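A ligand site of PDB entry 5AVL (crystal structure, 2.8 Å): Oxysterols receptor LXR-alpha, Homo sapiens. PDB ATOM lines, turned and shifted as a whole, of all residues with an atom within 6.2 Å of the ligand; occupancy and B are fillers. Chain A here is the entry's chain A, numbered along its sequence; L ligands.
O2 of the ligand is in hydrogen-bond range of N of Leu 152 (2.7 Å). The guanidinium group of Arg 141 lies within salt-bridge range of an oxygen (O4) of the ligand, 2.9 Å away. O3 of the ligand sits close to NE2 of His 257, 3.4 Å away.
The side-chain hydroxyl of Thr 138 is in hydrogen-bond range of the backbone carbonyl oxygen of Met 134 (2.8 Å). The backbone carbonyl oxygen (O) of Phe 90 lies within hydrogen-bond range of the side-chain hydroxyl (OG1) of Thr 94 (3.3 Å). The guanidinium group (NH1) of Arg 141 is in salt-bridge range of the side-chain carboxylate (OE1) of Glu 137 (2.5 Å). OG1 of Thr 150 lies within hydrogen-bond range of O of Arg 141 (2.9 Å). The backbone carbonyl oxygen (O) of Phe 162 lies within hydrogen-bond range of the backbone NH (N) of Leu 167 (3.4 Å).
Phe 90 touches the ligand. Phe 93 touches the ligand (O to C25, 3.3 Å). Thr 94 touches the ligand. CB of Leu 96 touches C4 of the ligand, 3.6 Å away. CB of Ala 97 touches O5 of the ligand, 3.5 Å away. Ser 100 touches the ligand. CD1 of Ile 131 touches O1 of the ligand (3.3 Å). CB of Met 134 touches C22 of the ligand, at 3.8 Å. Leu 135 touches the ligand (CD2 to C21, 3.7 Å). CB of Glu 137 touches C5 of the ligand, 3.997 Å away. Thr 138 touches the ligand (OG1 to C23, 3.3 Å). Phe 151 touches the ligand. CE2 of Phe 162 touches C23 of the ligand, 3.9 Å away. CD2 of Leu 167 touches F3 of the ligand, 3.3 Å away. CE2 of Phe 171 touches O3 of the ligand (3.4 Å). Ile 175 touches the ligand. CG of Gln 260 touches F3 of the ligand, 3.3 Å away. Leu 264 touches the ligand. Leu 271 touches the ligand (CD2 to F2, 3.6 Å). CZ3 of Trp 279 touches F2 of the ligand (3.5 Å). Hydrophobic or aromatic side chains that line the ligand: Phe 90, Phe 93, Leu 96, Ala 97, Ile 131, Met 134, Leu 135, Phe 151, Leu 152, Phe 162, Leu 167, Phe 171, Ile 175, His 257, Leu 264, Leu 271 and Trp 279. 23 residues have an atom within 4 Å of the ligand: Phe 90, Phe 93, Thr 94, Leu 96, Ala 97, Ser 100, Ile 131, Met 134, Leu 135, Glu 137, Thr 138, Arg 141, Phe 151, Leu 152, Phe 162, Leu 167, Phe 171, Ile 175, His 257, Gln 260, Leu 264, Leu 271 and Trp 279.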
ATOM      1  N   PHE A  90       5.635 -26.258 -18.110  1.00  0.00           N
ATOM      2  CA  PHE A  90       4.955 -25.238 -17.334  1.00  0.00           C
ATOM      3  C   PHE A  90       5.576 -25.131 -15.948  1.00  0.00           C
ATOM      4  O   PHE A  90       5.845 -24.025 -15.454  1.00  0.00           O
ATOM      5  CB  PHE A  90       3.475 -25.586 -17.240  1.00  0.00           C
ATOM      6  CG  PHE A  90       2.675 -24.667 -16.375  1.00  0.00           C
ATOM      7  CD1 PHE A  90       2.399 -23.361 -16.782  1.00  0.00           C
ATOM      8  CD2 PHE A  90       2.184 -25.105 -15.147  1.00  0.00           C
ATOM      9  CE1 PHE A  90       1.659 -22.509 -15.982  1.00  0.00           C
ATOM     10  CE2 PHE A  90       1.444 -24.252 -14.348  1.00  0.00           C
ATOM     11  CZ  PHE A  90       1.173 -22.961 -14.771  1.00  0.00           C
ATOM     12  N   PHE A  93       8.935 -23.338 -15.630  1.00  0.00           N
ATOM     13  CA  PHE A  93       8.799 -21.943 -15.949  1.00  0.00           C
ATOM     14  C   PHE A  93       8.313 -21.212 -14.730  1.00  0.00           C
ATOM     15  O   PHE A  93       8.830 -20.130 -14.412  1.00  0.00           O
ATOM     16  CB  PHE A  93       7.809 -21.743 -17.098  1.00  0.00           C
ATOM     17  CG  PHE A  93       8.102 -20.524 -17.935  1.00  0.00           C
ATOM     18  CD1 PHE A  93       9.416 -20.172 -18.241  1.00  0.00           C
ATOM     19  CD2 PHE A  93       7.074 -19.739 -18.417  1.00  0.00           C
ATOM     20  CE1 PHE A  93       9.708 -19.041 -19.015  1.00  0.00           C
ATOM     21  CE2 PHE A  93       7.346 -18.609 -19.195  1.00  0.00           C
ATOM     22  CZ  PHE A  93       8.670 -18.256 -19.499  1.00  0.00           C
ATOM     23  N   THR A  94       7.323 -21.802 -14.055  1.00  0.00           N
ATOM     24  CA  THR A  94       6.786 -21.249 -12.807  1.00  0.00           C
ATOM     25  C   THR A  94       7.807 -21.311 -11.683  1.00  0.00           C
ATOM     26  O   THR A  94       7.760 -20.483 -10.769  1.00  0.00           O
ATOM     27  CB  THR A  94       5.540 -21.975 -12.333  1.00  0.00           C
ATOM     28  OG1 THR A  94       5.804 -23.374 -12.246  1.00  0.00           O
ATOM     29  CG2 THR A  94       4.397 -21.745 -13.273  1.00  0.00           C
ATOM     30  N   LEU A  96      11.089 -20.829 -12.155  1.00  0.00           N
ATOM     31  CA  LEU A  96      11.903 -19.647 -12.410  1.00  0.00           C
ATOM     32  C   LEU A  96      11.275 -18.360 -11.854  1.00  0.00           C
ATOM     33  O   LEU A  96      11.991 -17.501 -11.338  1.00  0.00           O
ATOM     34  CB  LEU A  96      12.160 -19.513 -13.899  1.00  0.00           C
ATOM     35  CG  LEU A  96      13.179 -20.479 -14.466  1.00  0.00           C
ATOM     36  CD1 LEU A  96      13.149 -20.391 -15.994  1.00  0.00           C
ATOM     37  CD2 LEU A  96      14.564 -20.201 -13.891  1.00  0.00           C
ATOM     38  N   ALA A  97       9.959 -18.225 -11.969  1.00  0.00           N
ATOM     39  CA  ALA A  97       9.246 -17.092 -11.418  1.00  0.00           C
ATOM     40  C   ALA A  97       9.359 -17.103  -9.908  1.00  0.00           C
ATOM     41  O   ALA A  97       9.577 -16.047  -9.320  1.00  0.00           O
ATOM     42  CB  ALA A  97       7.784 -17.098 -11.843  1.00  0.00           C
ATOM     43  N   ILE A  98       9.238 -18.291  -9.279  1.00  0.00           N
ATOM     44  CA  ILE A  98       9.296 -18.396  -7.824  1.00  0.00           C
ATOM     45  C   ILE A  98      10.650 -17.890  -7.332  1.00  0.00           C
ATOM     46  O   ILE A  98      10.718 -17.035  -6.427  1.00  0.00           O
ATOM     47  CB  ILE A  98       9.042 -19.818  -7.331  1.00  0.00           C
ATOM     48  CG1 ILE A  98       7.575 -20.206  -7.498  1.00  0.00           C
ATOM     49  CG2 ILE A  98       9.387 -19.936  -5.865  1.00  0.00           C
ATOM     50  CD1 ILE A  98       7.345 -21.699  -7.353  1.00  0.00           C
ATOM     51  N   VAL A  99      11.710 -18.373  -7.980  1.00  0.00           N
ATOM     52  CA  VAL A  99      13.059 -17.882  -7.771  1.00  0.00           C
ATOM     53  C   VAL A  99      13.076 -16.369  -7.932  1.00  0.00           C
ATOM     54  O   VAL A  99      13.595 -15.666  -7.081  1.00  0.00           O
ATOM     55  CB  VAL A  99      14.107 -18.558  -8.726  1.00  0.00           C
ATOM     56  CG1 VAL A  99      15.455 -17.807  -8.769  1.00  0.00           C
ATOM     57  CG2 VAL A  99      14.315 -20.053  -8.387  1.00  0.00           C
ATOM     58  N   SER A 100      12.455 -15.868  -8.997  1.00  0.00           N
ATOM     59  CA  SER A 100      12.492 -14.443  -9.227  1.00  0.00           C
ATOM     60  C   SER A 100      11.825 -13.664  -8.075  1.00  0.00           C
ATOM     61  O   SER A 100      12.417 -12.704  -7.572  1.00  0.00           O
ATOM     62  CB  SER A 100      11.941 -14.057 -10.606  1.00  0.00           C
ATOM     63  OG  SER A 100      11.874 -12.640 -10.744  1.00  0.00           O
ATOM     64  N   GLU A 103      14.247 -13.165  -5.329  1.00  0.00           N
ATOM     65  CA  GLU A 103      15.203 -12.170  -5.716  1.00  0.00           C
ATOM     66  C   GLU A 103      14.655 -10.741  -5.564  1.00  0.00           C
ATOM     67  O   GLU A 103      15.299  -9.882  -4.962  1.00  0.00           O
ATOM     68  CB  GLU A 103      15.745 -12.461  -7.120  1.00  0.00           C
ATOM     69  CG  GLU A 103      16.929 -13.443  -7.124  1.00  0.00           C
ATOM     70  CD  GLU A 103      17.693 -13.526  -8.457  1.00  0.00           C
ATOM     71  OE1 GLU A 103      17.454 -12.687  -9.369  1.00  0.00           O
ATOM     72  OE2 GLU A 103      18.557 -14.414  -8.605  1.00  0.00           O
ATOM     73  N   ILE A 131       5.390  -8.794 -11.101  1.00  0.00           N
ATOM     74  CA  ILE A 131       5.308  -9.130 -12.511  1.00  0.00           C
ATOM     75  C   ILE A 131       6.026  -8.077 -13.331  1.00  0.00           C
ATOM     76  O   ILE A 131       6.727  -8.426 -14.311  1.00  0.00           O
ATOM     77  CB  ILE A 131       3.862  -9.329 -13.014  1.00  0.00           C
ATOM     78  CG1 ILE A 131       3.848  -9.661 -14.493  1.00  0.00           C
ATOM     79  CG2 ILE A 131       3.030  -8.078 -12.806  1.00  0.00           C
ATOM     80  CD1 ILE A 131       4.423 -11.006 -14.816  1.00  0.00           C
ATOM     81  N   MET A 134       9.621  -8.633 -13.037  1.00  0.00           N
ATOM     82  CA  MET A 134       9.881  -9.817 -13.835  1.00  0.00           C
ATOM     83  C   MET A 134       9.942  -9.493 -15.312  1.00  0.00           C
ATOM     84  O   MET A 134      10.798  -9.984 -16.052  1.00  0.00           O
ATOM     85  CB  MET A 134       8.805 -10.853 -13.585  1.00  0.00           C
ATOM     86  CG  MET A 134       8.919 -11.564 -12.259  1.00  0.00           C
ATOM     87  SD  MET A 134       7.394 -12.519 -12.085  1.00  0.00           S
ATOM     88  CE  MET A 134       7.729 -13.484 -10.645  1.00  0.00           C
ATOM     89  N   LEU A 135       9.046  -8.629 -15.759  1.00  0.00           N
ATOM     90  CA  LEU A 135       9.063  -8.213 -17.152  1.00  0.00           C
ATOM     91  C   LEU A 135      10.256  -7.300 -17.483  1.00  0.00           C
ATOM     92  O   LEU A 135      10.765  -7.323 -18.619  1.00  0.00           O
ATOM     93  CB  LEU A 135       7.729  -7.595 -17.534  1.00  0.00           C
ATOM     94  CG  LEU A 135       6.615  -8.612 -17.561  1.00  0.00           C
ATOM     95  CD1 LEU A 135       5.274  -7.902 -17.542  1.00  0.00           C
ATOM     96  CD2 LEU A 135       6.721  -9.556 -18.750  1.00  0.00           C
ATOM     97  N   GLU A 137      13.127  -7.662 -16.040  1.00  0.00           N
ATOM     98  CA  GLU A 137      14.232  -8.568 -16.029  1.00  0.00           C
ATOM     99  C   GLU A 137      14.191  -9.408 -17.310  1.00  0.00           C
ATOM    100  O   GLU A 137      15.236  -9.789 -17.828  1.00  0.00           O
ATOM    101  CB  GLU A 137      14.248  -9.489 -14.773  1.00  0.00           C
ATOM    102  CG  GLU A 137      14.495  -8.820 -13.421  1.00  0.00           C
ATOM    103  CD  GLU A 137      15.940  -8.412 -13.168  1.00  0.00           C
ATOM    104  OE1 GLU A 137      16.767  -8.500 -14.073  1.00  0.00           O
ATOM    105  OE2 GLU A 137      16.277  -7.987 -12.065  1.00  0.00           O
ATOM    106  N   THR A 138      12.985  -9.652 -17.817  1.00  0.00           N
ATOM    107  CA  THR A 138      12.816 -10.328 -19.106  1.00  0.00           C
ATOM    108  C   THR A 138      13.437  -9.495 -20.214  1.00  0.00           C
ATOM    109  O   THR A 138      14.300  -9.973 -20.945  1.00  0.00           O
ATOM    110  CB  THR A 138      11.335 -10.652 -19.397  1.00  0.00           C
ATOM    111  OG1 THR A 138      10.863 -11.551 -18.384  1.00  0.00           O
ATOM    112  CG2 THR A 138      11.166 -11.298 -20.778  1.00  0.00           C
ATOM    113  N   ARG A 141      17.381  -9.430 -20.498  1.00  0.00           N
ATOM    114  CA  ARG A 141      18.060 -10.539 -21.125  1.00  0.00           C
ATOM    115  C   ARG A 141      17.572 -10.944 -22.504  1.00  0.00           C
ATOM    116  O   ARG A 141      17.691 -12.112 -22.887  1.00  0.00           O
ATOM    117  CB  ARG A 141      18.102 -11.730 -20.191  1.00  0.00           C
ATOM    118  CG  ARG A 141      17.386 -11.525 -18.905  1.00  0.00           C
ATOM    119  CD  ARG A 141      18.157 -12.104 -17.722  1.00  0.00           C
ATOM    120  NE  ARG A 141      17.935 -11.225 -16.557  1.00  0.00           N
ATOM    121  CZ  ARG A 141      18.732 -11.129 -15.515  1.00  0.00           C
ATOM    122  NH1 ARG A 141      18.468 -10.277 -14.555  1.00  0.00           N
ATOM    123  NH2 ARG A 141      19.823 -11.863 -15.431  1.00  0.00           N
ATOM    124  N   THR A 150      17.321 -15.086 -22.587  1.00  0.00           N
ATOM    125  CA  THR A 150      18.343 -15.896 -21.900  1.00  0.00           C
ATOM    126  C   THR A 150      18.207 -15.734 -20.366  1.00  0.00           C
ATOM    127  O   THR A 150      18.793 -14.829 -19.746  1.00  0.00           O
ATOM    128  CB  THR A 150      19.775 -15.509 -22.407  1.00  0.00           C
ATOM    129  OG1 THR A 150      19.812 -14.104 -22.717  1.00  0.00           O
ATOM    130  CG2 THR A 150      20.190 -16.279 -23.666  1.00  0.00           C
ATOM    131  N   PHE A 151      17.394 -16.614 -19.780  1.00  0.00           N
ATOM    132  CA  PHE A 151      17.282 -16.770 -18.334  1.00  0.00           C
ATOM    133  C   PHE A 151      18.335 -17.737 -17.792  1.00  0.00           C
ATOM    134  O   PHE A 151      18.471 -18.872 -18.295  1.00  0.00           O
ATOM    135  CB  PHE A 151      15.916 -17.359 -17.943  1.00  0.00           C
ATOM    136  CG  PHE A 151      14.752 -16.463 -18.220  1.00  0.00           C
ATOM    137  CD1 PHE A 151      14.650 -15.204 -17.622  1.00  0.00           C
ATOM    138  CD2 PHE A 151      13.721 -16.895 -19.041  1.00  0.00           C
ATOM    139  CE1 PHE A 151      13.562 -14.373 -17.865  1.00  0.00           C
ATOM    140  CE2 PHE A 151      12.611 -16.092 -19.272  1.00  0.00           C
ATOM    141  CZ  PHE A 151      12.540 -14.834 -18.676  1.00  0.00           C
ATOM    142  N   LEU A 152      19.042 -17.307 -16.735  1.00  0.00           N
ATOM    143  CA  LEU A 152      20.064 -18.137 -16.044  1.00  0.00           C
ATOM    144  C   LEU A 152      21.111 -18.685 -16.976  1.00  0.00           C
ATOM    145  O   LEU A 152      21.134 -19.898 -17.203  1.00  0.00           O
ATOM    146  CB  LEU A 152      19.442 -19.283 -15.221  1.00  0.00           C
ATOM    147  CG  LEU A 152      19.188 -19.065 -13.718  1.00  0.00           C
ATOM    148  CD1 LEU A 152      20.194 -18.105 -13.102  1.00  0.00           C
ATOM    149  CD2 LEU A 152      17.782 -18.579 -13.431  1.00  0.00           C
ATOM    150  N   LYS A 153      21.944 -17.795 -17.517  1.00  0.00           N
ATOM    151  CA  LYS A 153      23.100 -18.085 -18.388  1.00  0.00           C
ATOM    152  C   LYS A 153      22.767 -18.946 -19.600  1.00  0.00           C
ATOM    153  O   LYS A 153      22.826 -18.503 -20.746  1.00  0.00           O
ATOM    154  CB  LYS A 153      24.250 -18.792 -17.651  1.00  0.00           C
ATOM    155  CG  LYS A 153      24.628 -18.271 -16.263  1.00  0.00           C
ATOM    156  CD  LYS A 153      25.514 -19.294 -15.528  1.00  0.00           C
ATOM    157  CE  LYS A 153      24.702 -20.314 -14.708  1.00  0.00           C
ATOM    158  NZ  LYS A 153      23.820 -19.611 -13.719  1.00  0.00           N
ATOM    159  N   PHE A 162       8.012 -20.174 -25.035  1.00  0.00           N
ATOM    160  CA  PHE A 162       7.079 -19.590 -24.072  1.00  0.00           C
ATOM    161  C   PHE A 162       5.708 -20.229 -24.210  1.00  0.00           C
ATOM    162  O   PHE A 162       5.051 -20.504 -23.220  1.00  0.00           O
ATOM    163  CB  PHE A 162       6.920 -18.103 -24.355  1.00  0.00           C
ATOM    164  CG  PHE A 162       7.830 -17.207 -23.579  1.00  0.00           C
ATOM    165  CD1 PHE A 162       9.213 -17.298 -23.711  1.00  0.00           C
ATOM    166  CD2 PHE A 162       7.288 -16.213 -22.774  1.00  0.00           C
ATOM    167  CE1 PHE A 162      10.032 -16.422 -23.026  1.00  0.00           C
ATOM    168  CE2 PHE A 162       8.112 -15.322 -22.070  1.00  0.00           C
ATOM    169  CZ  PHE A 162       9.495 -15.432 -22.198  1.00  0.00           C
ATOM    170  N   ALA A 165       5.755 -23.517 -22.845  1.00  0.00           N
ATOM    171  CA  ALA A 165       5.740 -23.353 -21.386  1.00  0.00           C
ATOM    172  C   ALA A 165       4.368 -22.991 -20.787  1.00  0.00           C
ATOM    173  O   ALA A 165       4.268 -22.772 -19.584  1.00  0.00           O
ATOM    174  CB  ALA A 165       6.788 -22.343 -20.951  1.00  0.00           C
ATOM    175  N   GLY A 166       3.327 -22.921 -21.611  1.00  0.00           N
ATOM    176  CA  GLY A 166       1.948 -22.856 -21.102  1.00  0.00           C
ATOM    177  C   GLY A 166       1.286 -21.502 -21.236  1.00  0.00           C
ATOM    178  O   GLY A 166       0.081 -21.359 -20.956  1.00  0.00           O
ATOM    179  N   LEU A 167       2.068 -20.504 -21.667  1.00  0.00           N
ATOM    180  CA  LEU A 167       1.558 -19.151 -21.794  1.00  0.00           C
ATOM    181  C   LEU A 167       0.875 -18.991 -23.143  1.00  0.00           C
ATOM    182  O   LEU A 167       1.225 -19.670 -24.101  1.00  0.00           O
ATOM    183  CB  LEU A 167       2.690 -18.151 -21.664  1.00  0.00           C
ATOM    184  CG  LEU A 167       3.654 -18.080 -20.458  1.00  0.00           C
ATOM    185  CD1 LEU A 167       4.330 -16.715 -20.421  1.00  0.00           C
ATOM    186  CD2 LEU A 167       2.958 -18.329 -19.135  1.00  0.00           C
ATOM    187  N   PHE A 171      -0.488 -12.976 -24.555  1.00  0.00           N
ATOM    188  CA  PHE A 171       0.505 -12.457 -23.585  1.00  0.00           C
ATOM    189  C   PHE A 171       1.944 -12.392 -24.194  1.00  0.00           C
ATOM    190  O   PHE A 171       2.624 -11.378 -24.031  1.00  0.00           O
ATOM    191  CB  PHE A 171       0.437 -13.307 -22.335  1.00  0.00           C
ATOM    192  CG  PHE A 171       1.276 -12.838 -21.191  1.00  0.00           C
ATOM    193  CD1 PHE A 171       1.545 -11.493 -20.954  1.00  0.00           C
ATOM    194  CD2 PHE A 171       1.750 -13.767 -20.253  1.00  0.00           C
ATOM    195  CE1 PHE A 171       2.305 -11.115 -19.850  1.00  0.00           C
ATOM    196  CE2 PHE A 171       2.512 -13.381 -19.161  1.00  0.00           C
ATOM    197  CZ  PHE A 171       2.800 -12.055 -18.957  1.00  0.00           C
ATOM    198  N   ILE A 175       4.721  -9.331 -24.509  1.00  0.00           N
ATOM    199  CA  ILE A 175       6.025  -9.478 -23.823  1.00  0.00           C
ATOM    200  C   ILE A 175       7.213  -9.216 -24.794  1.00  0.00           C
ATOM    201  O   ILE A 175       8.107  -8.401 -24.500  1.00  0.00           O
ATOM    202  CB  ILE A 175       6.206 -10.851 -23.181  1.00  0.00           C
ATOM    203  CG1 ILE A 175       5.192 -11.075 -22.080  1.00  0.00           C
ATOM    204  CG2 ILE A 175       7.592 -10.979 -22.543  1.00  0.00           C
ATOM    205  CD1 ILE A 175       4.914 -12.552 -21.866  1.00  0.00           C
ATOM    206  N   HIS A 257      -1.110  -9.779 -18.317  1.00  0.00           N
ATOM    207  CA  HIS A 257      -0.797 -10.848 -17.375  1.00  0.00           C
ATOM    208  C   HIS A 257      -2.001 -11.232 -16.485  1.00  0.00           C
ATOM    209  O   HIS A 257      -2.138 -12.402 -16.096  1.00  0.00           O
ATOM    210  CB  HIS A 257       0.438 -10.485 -16.573  1.00  0.00           C
ATOM    211  CG  HIS A 257       0.746 -11.471 -15.493  1.00  0.00           C
ATOM    212  ND1 HIS A 257       0.538 -11.199 -14.150  1.00  0.00           N
ATOM    213  CD2 HIS A 257       1.212 -12.742 -15.544  1.00  0.00           C
ATOM    214  CE1 HIS A 257       0.872 -12.248 -13.430  1.00  0.00           C
ATOM    215  NE2 HIS A 257       1.281 -13.202 -14.246  1.00  0.00           N
ATOM    216  N   GLN A 260      -4.008 -13.439 -18.515  1.00  0.00           N
ATOM    217  CA  GLN A 260      -3.277 -14.681 -18.560  1.00  0.00           C
ATOM    218  C   GLN A 260      -3.584 -15.594 -17.375  1.00  0.00           C
ATOM    219  O   GLN A 260      -3.881 -16.802 -17.556  1.00  0.00           O
ATOM    220  CB  GLN A 260      -1.767 -14.403 -18.641  1.00  0.00           C
ATOM    221  CG  GLN A 260      -0.871 -15.627 -18.734  1.00  0.00           C
ATOM    222  CD  GLN A 260      -1.132 -16.461 -19.955  1.00  0.00           C
ATOM    223  OE1 GLN A 260      -2.109 -17.207 -20.044  1.00  0.00           O
ATOM    224  NE2 GLN A 260      -0.240 -16.365 -20.908  1.00  0.00           N
ATOM    225  N   VAL A 261      -3.512 -15.021 -16.181  1.00  0.00           N
ATOM    226  CA  VAL A 261      -3.769 -15.735 -14.936  1.00  0.00           C
ATOM    227  C   VAL A 261      -5.184 -16.293 -14.945  1.00  0.00           C
ATOM    228  O   VAL A 261      -5.406 -17.469 -14.587  1.00  0.00           O
ATOM    229  CB  VAL A 261      -3.577 -14.825 -13.697  1.00  0.00           C
ATOM    230  CG1 VAL A 261      -4.076 -15.501 -12.436  1.00  0.00           C
ATOM    231  CG2 VAL A 261      -2.110 -14.437 -13.530  1.00  0.00           C
ATOM    232  N   LEU A 264      -5.694 -19.380 -17.274  1.00  0.00           N
ATOM    233  CA  LEU A 264      -5.144 -20.588 -16.695  1.00  0.00           C
ATOM    234  C   LEU A 264      -6.142 -21.242 -15.807  1.00  0.00           C
ATOM    235  O   LEU A 264      -6.145 -22.471 -15.709  1.00  0.00           O
ATOM    236  CB  LEU A 264      -3.930 -20.265 -15.846  1.00  0.00           C
ATOM    237  CG  LEU A 264      -2.663 -19.982 -16.634  1.00  0.00           C
ATOM    238  CD1 LEU A 264      -1.522 -19.697 -15.688  1.00  0.00           C
ATOM    239  CD2 LEU A 264      -2.345 -21.163 -17.546  1.00  0.00           C
ATOM    240  N   LEU A 271      -1.314 -22.542 -10.847  1.00  0.00           N
ATOM    241  CA  LEU A 271      -0.158 -21.835 -10.293  1.00  0.00           C
ATOM    242  C   LEU A 271       0.338 -22.473  -8.985  1.00  0.00           C
ATOM    243  O   LEU A 271      -0.459 -22.857  -8.163  1.00  0.00           O
ATOM    244  CB  LEU A 271      -0.526 -20.355 -10.045  1.00  0.00           C
ATOM    245  CG  LEU A 271      -0.839 -19.511 -11.293  1.00  0.00           C
ATOM    246  CD1 LEU A 271      -1.197 -18.051 -10.996  1.00  0.00           C
ATOM    247  CD2 LEU A 271       0.339 -19.594 -12.249  1.00  0.00           C
ATOM    248  N   LEU A 275       3.113 -18.226  -6.260  1.00  0.00           N
ATOM    249  CA  LEU A 275       2.668 -17.471  -7.414  1.00  0.00           C
ATOM    250  C   LEU A 275       1.170 -17.269  -7.295  1.00  0.00           C
ATOM    251  O   LEU A 275       0.656 -16.196  -7.569  1.00  0.00           O
ATOM    252  CB  LEU A 275       3.072 -18.141  -8.732  1.00  0.00           C
ATOM    253  CG  LEU A 275       4.551 -18.363  -9.073  1.00  0.00           C
ATOM    254  CD1 LEU A 275       4.689 -18.773 -10.528  1.00  0.00           C
ATOM    255  CD2 LEU A 275       5.377 -17.116  -8.780  1.00  0.00           C
ATOM    256  N   TRP A 279      -0.803 -13.754  -7.352  1.00  0.00           N
ATOM    257  CA  TRP A 279      -1.480 -13.503  -8.615  1.00  0.00           C
ATOM    258  C   TRP A 279      -2.904 -13.973  -8.731  1.00  0.00           C
ATOM    259  O   TRP A 279      -3.661 -13.410  -9.495  1.00  0.00           O
ATOM    260  CB  TRP A 279      -0.698 -14.097  -9.803  1.00  0.00           C
ATOM    261  CG  TRP A 279       0.610 -13.444 -10.054  1.00  0.00           C
ATOM    262  CD1 TRP A 279       0.968 -12.167  -9.748  1.00  0.00           C
ATOM    263  CD2 TRP A 279       1.741 -14.026 -10.725  1.00  0.00           C
ATOM    264  NE1 TRP A 279       2.260 -11.911 -10.163  1.00  0.00           N
ATOM    265  CE2 TRP A 279       2.750 -13.034 -10.771  1.00  0.00           C
ATOM    266  CE3 TRP A 279       1.994 -15.283 -11.308  1.00  0.00           C
ATOM    267  CZ2 TRP A 279       4.003 -13.252 -11.371  1.00  0.00           C
ATOM    268  CZ3 TRP A 279       3.235 -15.499 -11.900  1.00  0.00           C
ATOM    269  CH2 TRP A 279       4.227 -14.491 -11.922  1.00  0.00           C
HETATM  270  C1  LIG L   1      13.815 -13.743 -14.463  1.00  0.00           C
HETATM  271  C2  LIG L   1      14.345 -16.034 -14.174  1.00  0.00           C
HETATM  272  C3  LIG L   1      11.087 -14.634 -14.085  1.00  0.00           C
HETATM  273  C4  LIG L   1      11.651 -16.395 -15.582  1.00  0.00           C
HETATM  274  C5  LIG L   1      15.110 -13.347 -14.181  1.00  0.00           C
HETATM  275  C6  LIG L   1      15.635 -15.663 -13.867  1.00  0.00           C
HETATM  276  C7  LIG L   1       5.468 -18.385 -15.413  1.00  0.00           C
HETATM  277  C8  LIG L   1       4.099 -18.485 -15.349  1.00  0.00           C
HETATM  278  C9  LIG L   1       9.739 -14.881 -14.256  1.00  0.00           C
HETATM  279  C10 LIG L   1      10.307 -16.666 -15.768  1.00  0.00           C
HETATM  280  C11 LIG L   1      13.417 -15.062 -14.463  1.00  0.00           C
HETATM  281  C12 LIG L   1      12.043 -15.382 -14.729  1.00  0.00           C
HETATM  282  C13 LIG L   1       5.334 -16.092 -16.112  1.00  0.00           C
HETATM  283  C14 LIG L   1      16.024 -14.325 -13.873  1.00  0.00           C
HETATM  284  C15 LIG L   1       6.093 -17.205 -15.778  1.00  0.00           C
HETATM  285  C16 LIG L   1       3.359 -17.390 -15.674  1.00  0.00           C
HETATM  286  C17 LIG L   1       9.375 -15.903 -15.100  1.00  0.00           C
HETATM  287  C18 LIG L   1       3.964 -16.221 -16.041  1.00  0.00           C
HETATM  288  C19 LIG L   1       5.764 -14.742 -16.554  1.00  0.00           C
HETATM  289  C20 LIG L   1      18.322 -14.551 -14.581  1.00  0.00           C
HETATM  290  C21 LIG L   1       6.807 -13.226 -18.902  1.00  0.00           C
HETATM  291  C22 LIG L   1       8.122 -12.683 -16.833  1.00  0.00           C
HETATM  292  C23 LIG L   1       8.941 -14.237 -18.442  1.00  0.00           C
HETATM  293  C24 LIG L   1      17.424 -13.922 -13.557  1.00  0.00           C
HETATM  294  C25 LIG L   1       7.556 -17.345 -15.763  1.00  0.00           C
HETATM  295  C26 LIG L   1       1.916 -17.537 -15.596  1.00  0.00           C
HETATM  296  C27 LIG L   1       7.685 -13.741 -17.792  1.00  0.00           C
HETATM  297  O1  LIG L   1       4.978 -13.802 -16.484  1.00  0.00           O
HETATM  298  O2  LIG L   1      17.975 -15.055 -15.627  1.00  0.00           O
HETATM  299  O3  LIG L   1       3.178 -15.130 -16.344  1.00  0.00           O
HETATM  300  O4  LIG L   1      19.612 -14.496 -14.178  1.00  0.00           O
HETATM  301  O5  LIG L   1       8.035 -16.128 -15.221  1.00  0.00           O
HETATM  302  O6  LIG L   1       7.054 -14.799 -17.077  1.00  0.00           O
HETATM  303  F1  LIG L   1       1.629 -18.854 -15.717  1.00  0.00           F
HETATM  304  F2  LIG L   1       1.399 -16.982 -14.470  1.00  0.00           F
HETATM  305  F3  LIG L   1       1.231 -17.002 -16.610  1.00  0.00           F
